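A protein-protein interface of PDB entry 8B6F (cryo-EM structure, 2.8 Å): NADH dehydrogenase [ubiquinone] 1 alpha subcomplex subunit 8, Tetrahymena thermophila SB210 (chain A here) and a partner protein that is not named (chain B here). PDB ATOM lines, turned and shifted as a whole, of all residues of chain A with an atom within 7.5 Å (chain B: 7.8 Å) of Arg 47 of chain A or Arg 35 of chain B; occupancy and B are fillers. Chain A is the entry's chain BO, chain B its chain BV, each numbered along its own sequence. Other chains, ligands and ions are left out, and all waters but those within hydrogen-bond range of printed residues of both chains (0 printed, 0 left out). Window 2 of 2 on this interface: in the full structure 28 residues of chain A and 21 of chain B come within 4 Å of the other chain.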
ATOM      1  N   GLY A  41       5.409   1.786  -8.879  1.00  0.00           N
ATOM      2  CA  GLY A  41       4.215   1.949  -8.069  1.00  0.00           C
ATOM      3  C   GLY A  41       4.140   3.310  -7.408  1.00  0.00           C
ATOM      4  O   GLY A  41       3.066   3.908  -7.318  1.00  0.00           O
ATOM      5  N   ILE A  42       5.275   3.813  -6.925  1.00  0.00           N
ATOM      6  CA  ILE A  42       5.288   5.136  -6.309  1.00  0.00           C
ATOM      7  C   ILE A  42       4.889   6.195  -7.326  1.00  0.00           C
ATOM      8  O   ILE A  42       4.093   7.093  -7.027  1.00  0.00           O
ATOM      9  CB  ILE A  42       6.675   5.421  -5.699  1.00  0.00           C
ATOM     10  CG1 ILE A  42       6.890   4.558  -4.454  1.00  0.00           C
ATOM     11  CG2 ILE A  42       6.817   6.896  -5.339  1.00  0.00           C
ATOM     12  CD1 ILE A  42       8.318   4.547  -3.954  1.00  0.00           C
ATOM     13  N   GLU A  43       5.441   6.121  -8.538  1.00  0.00           N
ATOM     14  CA  GLU A  43       5.079   7.088  -9.568  1.00  0.00           C
ATOM     15  C   GLU A  43       3.590   7.023  -9.876  1.00  0.00           C
ATOM     16  O   GLU A  43       2.897   8.046  -9.878  1.00  0.00           O
ATOM     17  CB  GLU A  43       5.886   6.829 -10.838  1.00  0.00           C
ATOM     18  CG  GLU A  43       5.760   7.940 -11.868  1.00  0.00           C
ATOM     19  CD  GLU A  43       6.116   7.490 -13.270  1.00  0.00           C
ATOM     20  OE1 GLU A  43       6.101   6.271 -13.531  1.00  0.00           O
ATOM     21  OE2 GLU A  43       6.411   8.359 -14.118  1.00  0.00           O
ATOM     22  N   GLN A  44       3.082   5.820 -10.153  1.00  0.00           N
ATOM     23  CA  GLN A  44       1.683   5.679 -10.537  1.00  0.00           C
ATOM     24  C   GLN A  44       0.762   6.121  -9.411  1.00  0.00           C
ATOM     25  O   GLN A  44      -0.250   6.790  -9.650  1.00  0.00           O
ATOM     26  CB  GLN A  44       1.393   4.231 -10.930  1.00  0.00           C
ATOM     27  CG  GLN A  44       2.212   3.736 -12.112  1.00  0.00           C
ATOM     28  CD  GLN A  44       1.899   4.472 -13.396  1.00  0.00           C
ATOM     29  OE1 GLN A  44       0.882   5.153 -13.504  1.00  0.00           O
ATOM     30  NE2 GLN A  44       2.780   4.342 -14.380  1.00  0.00           N
ATOM     31  N   CYS A  45       1.096   5.756  -8.172  1.00  0.00           N
ATOM     32  CA  CYS A  45       0.266   6.142  -7.039  1.00  0.00           C
ATOM     33  C   CYS A  45       0.342   7.638  -6.771  1.00  0.00           C
ATOM     34  O   CYS A  45      -0.658   8.242  -6.370  1.00  0.00           O
ATOM     35  CB  CYS A  45       0.679   5.362  -5.792  1.00  0.00           C
ATOM     36  SG  CYS A  45      -0.386   5.648  -4.365  1.00  0.00           S
ATOM     37  N   ARG A  46       1.502   8.258  -6.991  1.00  0.00           N
ATOM     38  CA  ARG A  46       1.587   9.708  -6.859  1.00  0.00           C
ATOM     39  C   ARG A  46       0.645  10.396  -7.838  1.00  0.00           C
ATOM     40  O   ARG A  46      -0.112  11.297  -7.462  1.00  0.00           O
ATOM     41  CB  ARG A  46       3.030  10.168  -7.074  1.00  0.00           C
ATOM     42  CG  ARG A  46       3.227  11.668  -6.913  1.00  0.00           C
ATOM     43  CD  ARG A  46       4.674  12.073  -7.125  1.00  0.00           C
ATOM     44  NE  ARG A  46       5.119  11.828  -8.491  1.00  0.00           N
ATOM     45  CZ  ARG A  46       6.269  12.254  -8.994  1.00  0.00           C
ATOM     46  NH1 ARG A  46       7.121  12.960  -8.269  1.00  0.00           N
ATOM     47  NH2 ARG A  46       6.573  11.966 -10.255  1.00  0.00           N
ATOM     48  N   ARG A  47       0.680   9.986  -9.107  1.00  0.00           N
ATOM     49  CA  ARG A  47      -0.218  10.577 -10.095  1.00  0.00           C
ATOM     50  C   ARG A  47      -1.674  10.312  -9.735  1.00  0.00           C
ATOM     51  O   ARG A  47      -2.525  11.200  -9.854  1.00  0.00           O
ATOM     52  CB  ARG A  47       0.104  10.035 -11.488  1.00  0.00           C
ATOM     53  CG  ARG A  47      -0.877  10.459 -12.574  1.00  0.00           C
ATOM     54  CD  ARG A  47      -1.068  11.967 -12.627  1.00  0.00           C
ATOM     55  NE  ARG A  47       0.181  12.673 -12.894  1.00  0.00           N
ATOM     56  CZ  ARG A  47       0.622  13.002 -14.101  1.00  0.00           C
ATOM     57  NH1 ARG A  47      -0.054  12.691 -15.194  1.00  0.00           N
ATOM     58  NH2 ARG A  47       1.771  13.660 -14.213  1.00  0.00           N
ATOM     59  N   LYS A  48      -1.975   9.091  -9.289  1.00  0.00           N
ATOM     60  CA  LYS A  48      -3.346   8.737  -8.938  1.00  0.00           C
ATOM     61  C   LYS A  48      -3.859   9.586  -7.782  1.00  0.00           C
ATOM     62  O   LYS A  48      -4.990  10.082  -7.822  1.00  0.00           O
ATOM     63  CB  LYS A  48      -3.421   7.251  -8.588  1.00  0.00           C
ATOM     64  CG  LYS A  48      -4.805   6.761  -8.187  1.00  0.00           C
ATOM     65  CD  LYS A  48      -4.752   5.318  -7.707  1.00  0.00           C
ATOM     66  CE  LYS A  48      -6.102   4.854  -7.184  1.00  0.00           C
ATOM     67  NZ  LYS A  48      -6.045   3.457  -6.666  1.00  0.00           N
ATOM     68  N   MET A  49      -3.044   9.765  -6.742  1.00  0.00           N
ATOM     69  CA  MET A  49      -3.472  10.574  -5.605  1.00  0.00           C
ATOM     70  C   MET A  49      -3.669  12.031  -6.004  1.00  0.00           C
ATOM     71  O   MET A  49      -4.628  12.673  -5.565  1.00  0.00           O
ATOM     72  CB  MET A  49      -2.455  10.467  -4.470  1.00  0.00           C
ATOM     73  CG  MET A  49      -2.326   9.077  -3.856  1.00  0.00           C
ATOM     74  SD  MET A  49      -3.880   8.400  -3.249  1.00  0.00           S
ATOM     75  CE  MET A  49      -4.409   7.422  -4.652  1.00  0.00           C
ATOM     76  N   VAL A  50      -2.773  12.575  -6.829  1.00  0.00           N
ATOM     77  CA  VAL A  50      -2.937  13.956  -7.275  1.00  0.00           C
ATOM     78  C   VAL A  50      -4.236  14.110  -8.055  1.00  0.00           C
ATOM     79  O   VAL A  50      -4.974  15.086  -7.873  1.00  0.00           O
ATOM     80  CB  VAL A  50      -1.718  14.400  -8.106  1.00  0.00           C
ATOM     81  CG1 VAL A  50      -1.979  15.747  -8.771  1.00  0.00           C
ATOM     82  CG2 VAL A  50      -0.481  14.475  -7.229  1.00  0.00           C
ATOM     83  N   GLN A  51      -4.539  13.155  -8.936  1.00  0.00           N
ATOM     84  CA  GLN A  51      -5.792  13.221  -9.680  1.00  0.00           C
ATOM     85  C   GLN A  51      -6.991  13.134  -8.745  1.00  0.00           C
ATOM     86  O   GLN A  51      -7.967  13.875  -8.903  1.00  0.00           O
ATOM     87  CB  GLN A  51      -5.847  12.101 -10.720  1.00  0.00           C
ATOM     88  CG  GLN A  51      -4.893  12.290 -11.884  1.00  0.00           C
ATOM     89  CD  GLN A  51      -4.978  11.164 -12.891  1.00  0.00           C
ATOM     90  OE1 GLN A  51      -5.673  10.173 -12.673  1.00  0.00           O
ATOM     91  NE2 GLN A  51      -4.271  11.313 -14.006  1.00  0.00           N
ATOM     92  N   LEU A  52      -6.938  12.230  -7.768  1.00  0.00           N
ATOM     93  CA  LEU A  52      -8.100  11.987  -6.921  1.00  0.00           C
ATOM     94  C   LEU A  52      -8.375  13.173  -6.003  1.00  0.00           C
ATOM     95  O   LEU A  52      -9.511  13.651  -5.919  1.00  0.00           O
ATOM     96  CB  LEU A  52      -7.886  10.708  -6.109  1.00  0.00           C
ATOM     97  CG  LEU A  52      -9.115  10.028  -5.494  1.00  0.00           C
ATOM     98  CD1 LEU A  52      -8.746   8.640  -5.005  1.00  0.00           C
ATOM     99  CD2 LEU A  52      -9.722  10.835  -4.352  1.00  0.00           C
ATOM    100  N   ALA A  53      -7.343  13.671  -5.317  1.00  0.00           N
ATOM    101  CA  ALA A  53      -7.511  14.698  -4.294  1.00  0.00           C
ATOM    102  C   ALA A  53      -6.701  15.954  -4.587  1.00  0.00           C
ATOM    103  O   ALA A  53      -6.446  16.747  -3.677  1.00  0.00           O
ATOM    104  CB  ALA A  53      -7.132  14.142  -2.920  1.00  0.00           C
ATOM    105  N   GLY A  54      -6.290  16.156  -5.839  1.00  0.00           N
ATOM    106  CA  GLY A  54      -5.542  17.356  -6.169  1.00  0.00           C
ATOM    107  C   GLY A  54      -6.332  18.624  -5.908  1.00  0.00           C
ATOM    108  O   GLY A  54      -5.783  19.624  -5.440  1.00  0.00           O
ATOM    109  N   PHE A  65      -1.102  11.905  -0.345  1.00  0.00           N
ATOM    110  CA  PHE A  65       0.081  11.061  -0.481  1.00  0.00           C
ATOM    111  C   PHE A  65       0.272  10.094   0.680  1.00  0.00           C
ATOM    112  O   PHE A  65       1.252   9.342   0.677  1.00  0.00           O
ATOM    113  CB  PHE A  65       1.364  11.889  -0.645  1.00  0.00           C
ATOM    114  CG  PHE A  65       1.406  12.700  -1.911  1.00  0.00           C
ATOM    115  CD1 PHE A  65       1.000  12.150  -3.117  1.00  0.00           C
ATOM    116  CD2 PHE A  65       1.844  14.012  -1.893  1.00  0.00           C
ATOM    117  CE1 PHE A  65       1.036  12.893  -4.278  1.00  0.00           C
ATOM    118  CE2 PHE A  65       1.882  14.760  -3.051  1.00  0.00           C
ATOM    119  CZ  PHE A  65       1.477  14.200  -4.246  1.00  0.00           C
ATOM    120  N   CYS A  68       0.683   6.615  -0.510  1.00  0.00           N
ATOM    121  CA  CYS A  68       2.028   6.347  -1.005  1.00  0.00           C
ATOM    122  C   CYS A  68       2.992   5.952   0.104  1.00  0.00           C
ATOM    123  O   CYS A  68       4.086   5.465  -0.197  1.00  0.00           O
ATOM    124  CB  CYS A  68       2.582   7.571  -1.737  1.00  0.00           C
ATOM    125  SG  CYS A  68       1.663   8.049  -3.211  1.00  0.00           S
ATOM    126  N   GLU B  28       1.508  24.174  -7.875  1.00  0.00           N
ATOM    127  CA  GLU B  28       2.370  23.031  -8.153  1.00  0.00           C
ATOM    128  C   GLU B  28       1.548  21.790  -8.478  1.00  0.00           C
ATOM    129  O   GLU B  28       1.883  21.038  -9.399  1.00  0.00           O
ATOM    130  CB  GLU B  28       3.284  22.764  -6.959  1.00  0.00           C
ATOM    131  CG  GLU B  28       4.164  23.941  -6.572  1.00  0.00           C
ATOM    132  CD  GLU B  28       5.229  24.243  -7.607  1.00  0.00           C
ATOM    133  OE1 GLU B  28       5.361  23.462  -8.571  1.00  0.00           O
ATOM    134  OE2 GLU B  28       5.935  25.260  -7.455  1.00  0.00           O
ATOM    135  N   LEU B  29       0.471  21.555  -7.727  1.00  0.00           N
ATOM    136  CA  LEU B  29      -0.388  20.412  -8.010  1.00  0.00           C
ATOM    137  C   LEU B  29      -0.990  20.511  -9.404  1.00  0.00           C
ATOM    138  O   LEU B  29      -1.036  19.518 -10.140  1.00  0.00           O
ATOM    139  CB  LEU B  29      -1.493  20.308  -6.958  1.00  0.00           C
ATOM    140  CG  LEU B  29      -1.113  19.684  -5.614  1.00  0.00           C
ATOM    141  CD1 LEU B  29      -2.261  19.807  -4.634  1.00  0.00           C
ATOM    142  CD2 LEU B  29      -0.722  18.224  -5.785  1.00  0.00           C
ATOM    143  N   GLU B  30      -1.457  21.699  -9.786  1.00  0.00           N
ATOM    144  CA  GLU B  30      -2.041  21.867 -11.112  1.00  0.00           C
ATOM    145  C   GLU B  30      -1.009  21.628 -12.206  1.00  0.00           C
ATOM    146  O   GLU B  30      -1.303  20.970 -13.211  1.00  0.00           O
ATOM    147  CB  GLU B  30      -2.645  23.263 -11.242  1.00  0.00           C
ATOM    148  CG  GLU B  30      -3.902  23.473 -10.414  1.00  0.00           C
ATOM    149  CD  GLU B  30      -5.062  22.621 -10.889  1.00  0.00           C
ATOM    150  OE1 GLU B  30      -4.984  22.080 -12.012  1.00  0.00           O
ATOM    151  OE2 GLU B  30      -6.050  22.489 -10.138  1.00  0.00           O
ATOM    152  N   ARG B  31       0.205  22.156 -12.038  1.00  0.00           N
ATOM    153  CA  ARG B  31       1.245  21.932 -13.036  1.00  0.00           C
ATOM    154  C   ARG B  31       1.558  20.449 -13.174  1.00  0.00           C
ATOM    155  O   ARG B  31       1.682  19.927 -14.287  1.00  0.00           O
ATOM    156  CB  ARG B  31       2.507  22.707 -12.661  1.00  0.00           C
ATOM    157  CG  ARG B  31       2.362  24.212 -12.744  1.00  0.00           C
ATOM    158  CD  ARG B  31       3.698  24.901 -12.527  1.00  0.00           C
ATOM    159  NE  ARG B  31       3.534  26.330 -12.287  1.00  0.00           N
ATOM    160  CZ  ARG B  31       3.418  26.886 -11.089  1.00  0.00           C
ATOM    161  NH1 ARG B  31       3.453  26.164  -9.982  1.00  0.00           N
ATOM    162  NH2 ARG B  31       3.263  28.204 -11.000  1.00  0.00           N
ATOM    163  N   PHE B  32       1.694  19.751 -12.046  1.00  0.00           N
ATOM    164  CA  PHE B  32       1.981  18.321 -12.090  1.00  0.00           C
ATOM    165  C   PHE B  32       0.846  17.553 -12.751  1.00  0.00           C
ATOM    166  O   PHE B  32       1.085  16.648 -13.558  1.00  0.00           O
ATOM    167  CB  PHE B  32       2.231  17.800 -10.677  1.00  0.00           C
ATOM    168  CG  PHE B  32       2.484  16.322 -10.609  1.00  0.00           C
ATOM    169  CD1 PHE B  32       3.729  15.805 -10.917  1.00  0.00           C
ATOM    170  CD2 PHE B  32       1.482  15.452 -10.221  1.00  0.00           C
ATOM    171  CE1 PHE B  32       3.967  14.450 -10.847  1.00  0.00           C
ATOM    172  CE2 PHE B  32       1.713  14.096 -10.149  1.00  0.00           C
ATOM    173  CZ  PHE B  32       2.957  13.593 -10.463  1.00  0.00           C
ATOM    174  N   LEU B  33      -0.399  17.901 -12.420  1.00  0.00           N
ATOM    175  CA  LEU B  33      -1.540  17.200 -12.999  1.00  0.00           C
ATOM    176  C   LEU B  33      -1.601  17.392 -14.509  1.00  0.00           C
ATOM    177  O   LEU B  33      -1.833  16.434 -15.254  1.00  0.00           O
ATOM    178  CB  LEU B  33      -2.832  17.689 -12.345  1.00  0.00           C
ATOM    179  CG  LEU B  33      -4.134  17.112 -12.903  1.00  0.00           C
ATOM    180  CD1 LEU B  33      -4.171  15.606 -12.738  1.00  0.00           C
ATOM    181  CD2 LEU B  33      -5.331  17.752 -12.228  1.00  0.00           C
ATOM    182  N   ASN B  34      -1.393  18.619 -14.977  1.00  0.00           N
ATOM    183  CA  ASN B  34      -1.502  18.934 -16.394  1.00  0.00           C
ATOM    184  C   ASN B  34      -0.213  18.682 -17.162  1.00  0.00           C
ATOM    185  O   ASN B  34      -0.187  18.894 -18.379  1.00  0.00           O
ATOM    186  CB  ASN B  34      -1.922  20.396 -16.575  1.00  0.00           C
ATOM    187  CG  ASN B  34      -3.313  20.671 -16.045  1.00  0.00           C
ATOM    188  OD1 ASN B  34      -4.185  19.805 -16.079  1.00  0.00           O
ATOM    189  ND2 ASN B  34      -3.529  21.888 -15.555  1.00  0.00           N
ATOM    190  N   ARG B  35       0.852  18.237 -16.495  1.00  0.00           N
ATOM    191  CA  ARG B  35       2.135  17.985 -17.149  1.00  0.00           C
ATOM    192  C   ARG B  35       2.700  19.257 -17.774  1.00  0.00           C
ATOM    193  O   ARG B  35       3.396  19.205 -18.790  1.00  0.00           O
ATOM    194  CB  ARG B  35       2.015  16.886 -18.208  1.00  0.00           C
ATOM    195  CG  ARG B  35       1.599  15.535 -17.657  1.00  0.00           C
ATOM    196  CD  ARG B  35       1.444  14.517 -18.777  1.00  0.00           C
ATOM    197  NE  ARG B  35       1.118  13.190 -18.268  1.00  0.00           N
ATOM    198  CZ  ARG B  35       2.011  12.286 -17.887  1.00  0.00           C
ATOM    199  NH1 ARG B  35       3.310  12.532 -17.940  1.00  0.00           N
ATOM    200  NH2 ARG B  35       1.590  11.107 -17.441  1.00  0.00           N
ATOM    201  N   GLU B  36       2.406  20.407 -17.170  1.00  0.00           N
ATOM    202  CA  GLU B  36       2.856  21.701 -17.667  1.00  0.00           C
ATOM    203  C   GLU B  36       3.901  22.329 -16.751  1.00  0.00           C
ATOM    204  O   GLU B  36       3.945  23.551 -16.594  1.00  0.00           O
ATOM    205  CB  GLU B  36       1.666  22.643 -17.844  1.00  0.00           C
ATOM    206  CG  GLU B  36       0.610  22.111 -18.800  1.00  0.00           C
ATOM    207  CD  GLU B  36      -0.522  23.093 -19.027  1.00  0.00           C
ATOM    208  OE1 GLU B  36      -0.494  24.184 -18.421  1.00  0.00           O
ATOM    209  OE2 GLU B  36      -1.439  22.774 -19.813  1.00  0.00           O
ATOM    210  N   GLN B  37       4.747  21.501 -16.136  1.00  0.00           N
ATOM    211  CA  GLN B  37       5.787  22.028 -15.259  1.00  0.00           C
ATOM    212  C   GLN B  37       6.796  22.865 -16.034  1.00  0.00           C
ATOM    213  O   GLN B  37       7.247  23.908 -15.549  1.00  0.00           O
ATOM    214  CB  GLN B  37       6.486  20.881 -14.530  1.00  0.00           C
ATOM    215  CG  GLN B  37       5.570  20.101 -13.604  1.00  0.00           C
ATOM    216  CD  GLN B  37       6.305  19.041 -12.813  1.00  0.00           C
ATOM    217  OE1 GLN B  37       7.506  18.839 -12.989  1.00  0.00           O
ATOM    218  NE2 GLN B  37       5.587  18.358 -11.931  1.00  0.00           N
ATOM    219  N   THR B  38       7.163  22.427 -17.237  1.00  0.00           N
ATOM    220  CA  THR B  38       8.140  23.119 -18.067  1.00  0.00           C
ATOM    221  C   THR B  38       7.516  23.779 -19.286  1.00  0.00           C
ATOM    222  O   THR B  38       7.775  24.957 -19.551  1.00  0.00           O
ATOM    223  CB  THR B  38       9.238  22.141 -18.512  1.00  0.00           C
ATOM    224  OG1 THR B  38       8.640  20.997 -19.135  1.00  0.00           O
ATOM    225  CG2 THR B  38      10.071  21.695 -17.321  1.00  0.00           C
ATOM    226  N   LEU B  39       6.696  23.050 -20.039  1.00  0.00           N
ATOM    227  CA  LEU B  39       6.061  23.570 -21.240  1.00  0.00           C
ATOM    228  C   LEU B  39       4.572  23.265 -21.197  1.00  0.00           C
ATOM    229  O   LEU B  39       4.146  22.240 -20.660  1.00  0.00           O
ATOM    230  CB  LEU B  39       6.682  22.964 -22.507  1.00  0.00           C
ATOM    231  CG  LEU B  39       8.173  23.242 -22.708  1.00  0.00           C
ATOM    232  CD1 LEU B  39       8.699  22.480 -23.906  1.00  0.00           C
ATOM    233  CD2 LEU B  39       8.431  24.732 -22.876  1.00  0.00           C
ATOM    234  N   THR B  40       3.784  24.164 -21.778  1.00  0.00           N
ATOM    235  CA  THR B  40       2.335  24.037 -21.786  1.00  0.00           C
ATOM    236  C   THR B  40       1.874  23.288 -23.029  1.00  0.00           C
ATOM    237  O   THR B  40       2.495  23.363 -24.091  1.00  0.00           O
ATOM    238  CB  THR B  40       1.659  25.410 -21.737  1.00  0.00           C
ATOM    239  OG1 THR B  40       2.163  26.235 -22.795  1.00  0.00           O
ATOM    240  CG2 THR B  40       1.917  26.086 -20.404  1.00  0.00           C
ATOM    241  N   VAL B  41       0.763  22.565 -22.883  1.00  0.00           N
ATOM    242  CA  VAL B  41       0.193  21.839 -24.014  1.00  0.00           C
ATOM    243  C   VAL B  41      -0.143  22.797 -25.143  1.00  0.00           C
ATOM    244  O   VAL B  41      -0.069  22.431 -26.322  1.00  0.00           O
ATOM    245  CB  VAL B  41      -1.043  21.035 -23.567  1.00  0.00           C
ATOM    246  CG1 VAL B  41      -1.671  20.311 -24.751  1.00  0.00           C
ATOM    247  CG2 VAL B  41      -0.665  20.043 -22.481  1.00  0.00           C
ATOM    248  N   HIS B  44       2.982  23.322 -27.048  1.00  0.00           N
ATOM    249  CA  HIS B  44       3.200  22.178 -27.926  1.00  0.00           C
ATOM    250  C   HIS B  44       2.310  22.262 -29.158  1.00  0.00           C
ATOM    251  O   HIS B  44       2.762  22.009 -30.280  1.00  0.00           O
ATOM    252  CB  HIS B  44       2.937  20.876 -27.172  1.00  0.00           C
ATOM    253  CG  HIS B  44       3.964  20.561 -26.132  1.00  0.00           C
ATOM    254  ND1 HIS B  44       5.129  19.884 -26.421  1.00  0.00           N
ATOM    255  CD2 HIS B  44       4.005  20.830 -24.807  1.00  0.00           C
ATOM    256  CE1 HIS B  44       5.842  19.750 -25.317  1.00  0.00           C
ATOM    257  NE2 HIS B  44       5.183  20.316 -24.323  1.00  0.00           N
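O of Phe 32 of chain B is in hydrogen-bond range of NH2 of Arg 47 of chain A (3.1 Å).
NH2 of Arg 35 of chain B lies close to NH1 of Arg 47 of chain A (3.2 Å).
Among the printed residues, pairs that only touch across the chains: Arg 46 of chain A with Phe 32 of chain B (3.4 Å), Val 50 of chain A with Phe 32 of chain B (3.7 Å), Gln 51 of chain A with Leu 33 of chain B (3.5 Å) and Gly 54 of chain A with Leu 29 of chain B (3.6 Å).
Of the printed residues of chain B, Gln 51 of chain A touches Leu 33 (3.5 Å).
Of the printed residues of chain B, Gly 54 of chain A touches Leu 29 (3.6 Å).
Of the printed residues of chain A, Phe 32 of chain B touches Arg 46 (3.4 Å), Arg 47 (3.1 Å) and Val 50 (3.7 Å).
Arg 35 of chain B touches just one residue of chain A: Arg 47.
The nearest residue of chain A that does not touch Arg 35 of chain B is Glu 43 of chain A (6.5 Å).
The nearest printed residue of chain A that does not touch Leu 33 of chain B is Arg 47 of chain A (4.1 Å).
N of Arg 46 of chain A is in hydrogen-bond range of SG of Cys 68 of chain A, 3.8 Å away.
Printed residues of chain B that touch a printed residue of chain A: Leu 29, Phe 32, Leu 33 and Arg 35.
Of the 16 printed residues of chain A, 5 touch a printed residue of chain B.
Printed residues of chain A that touch a printed residue of chain B: Arg 46, Arg 47, Val 50, Gln 51 and Gly 54.
Hydrophobic or aromatic side chains of chain A that line the printed part of chain B: Val 50.
Among the printed residues, 6 pairs touch across the chains.
Among the printed residues, no Asp or Glu carboxylate lies within 4 Å of a Lys or Arg side-chain nitrogen of the other chain.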
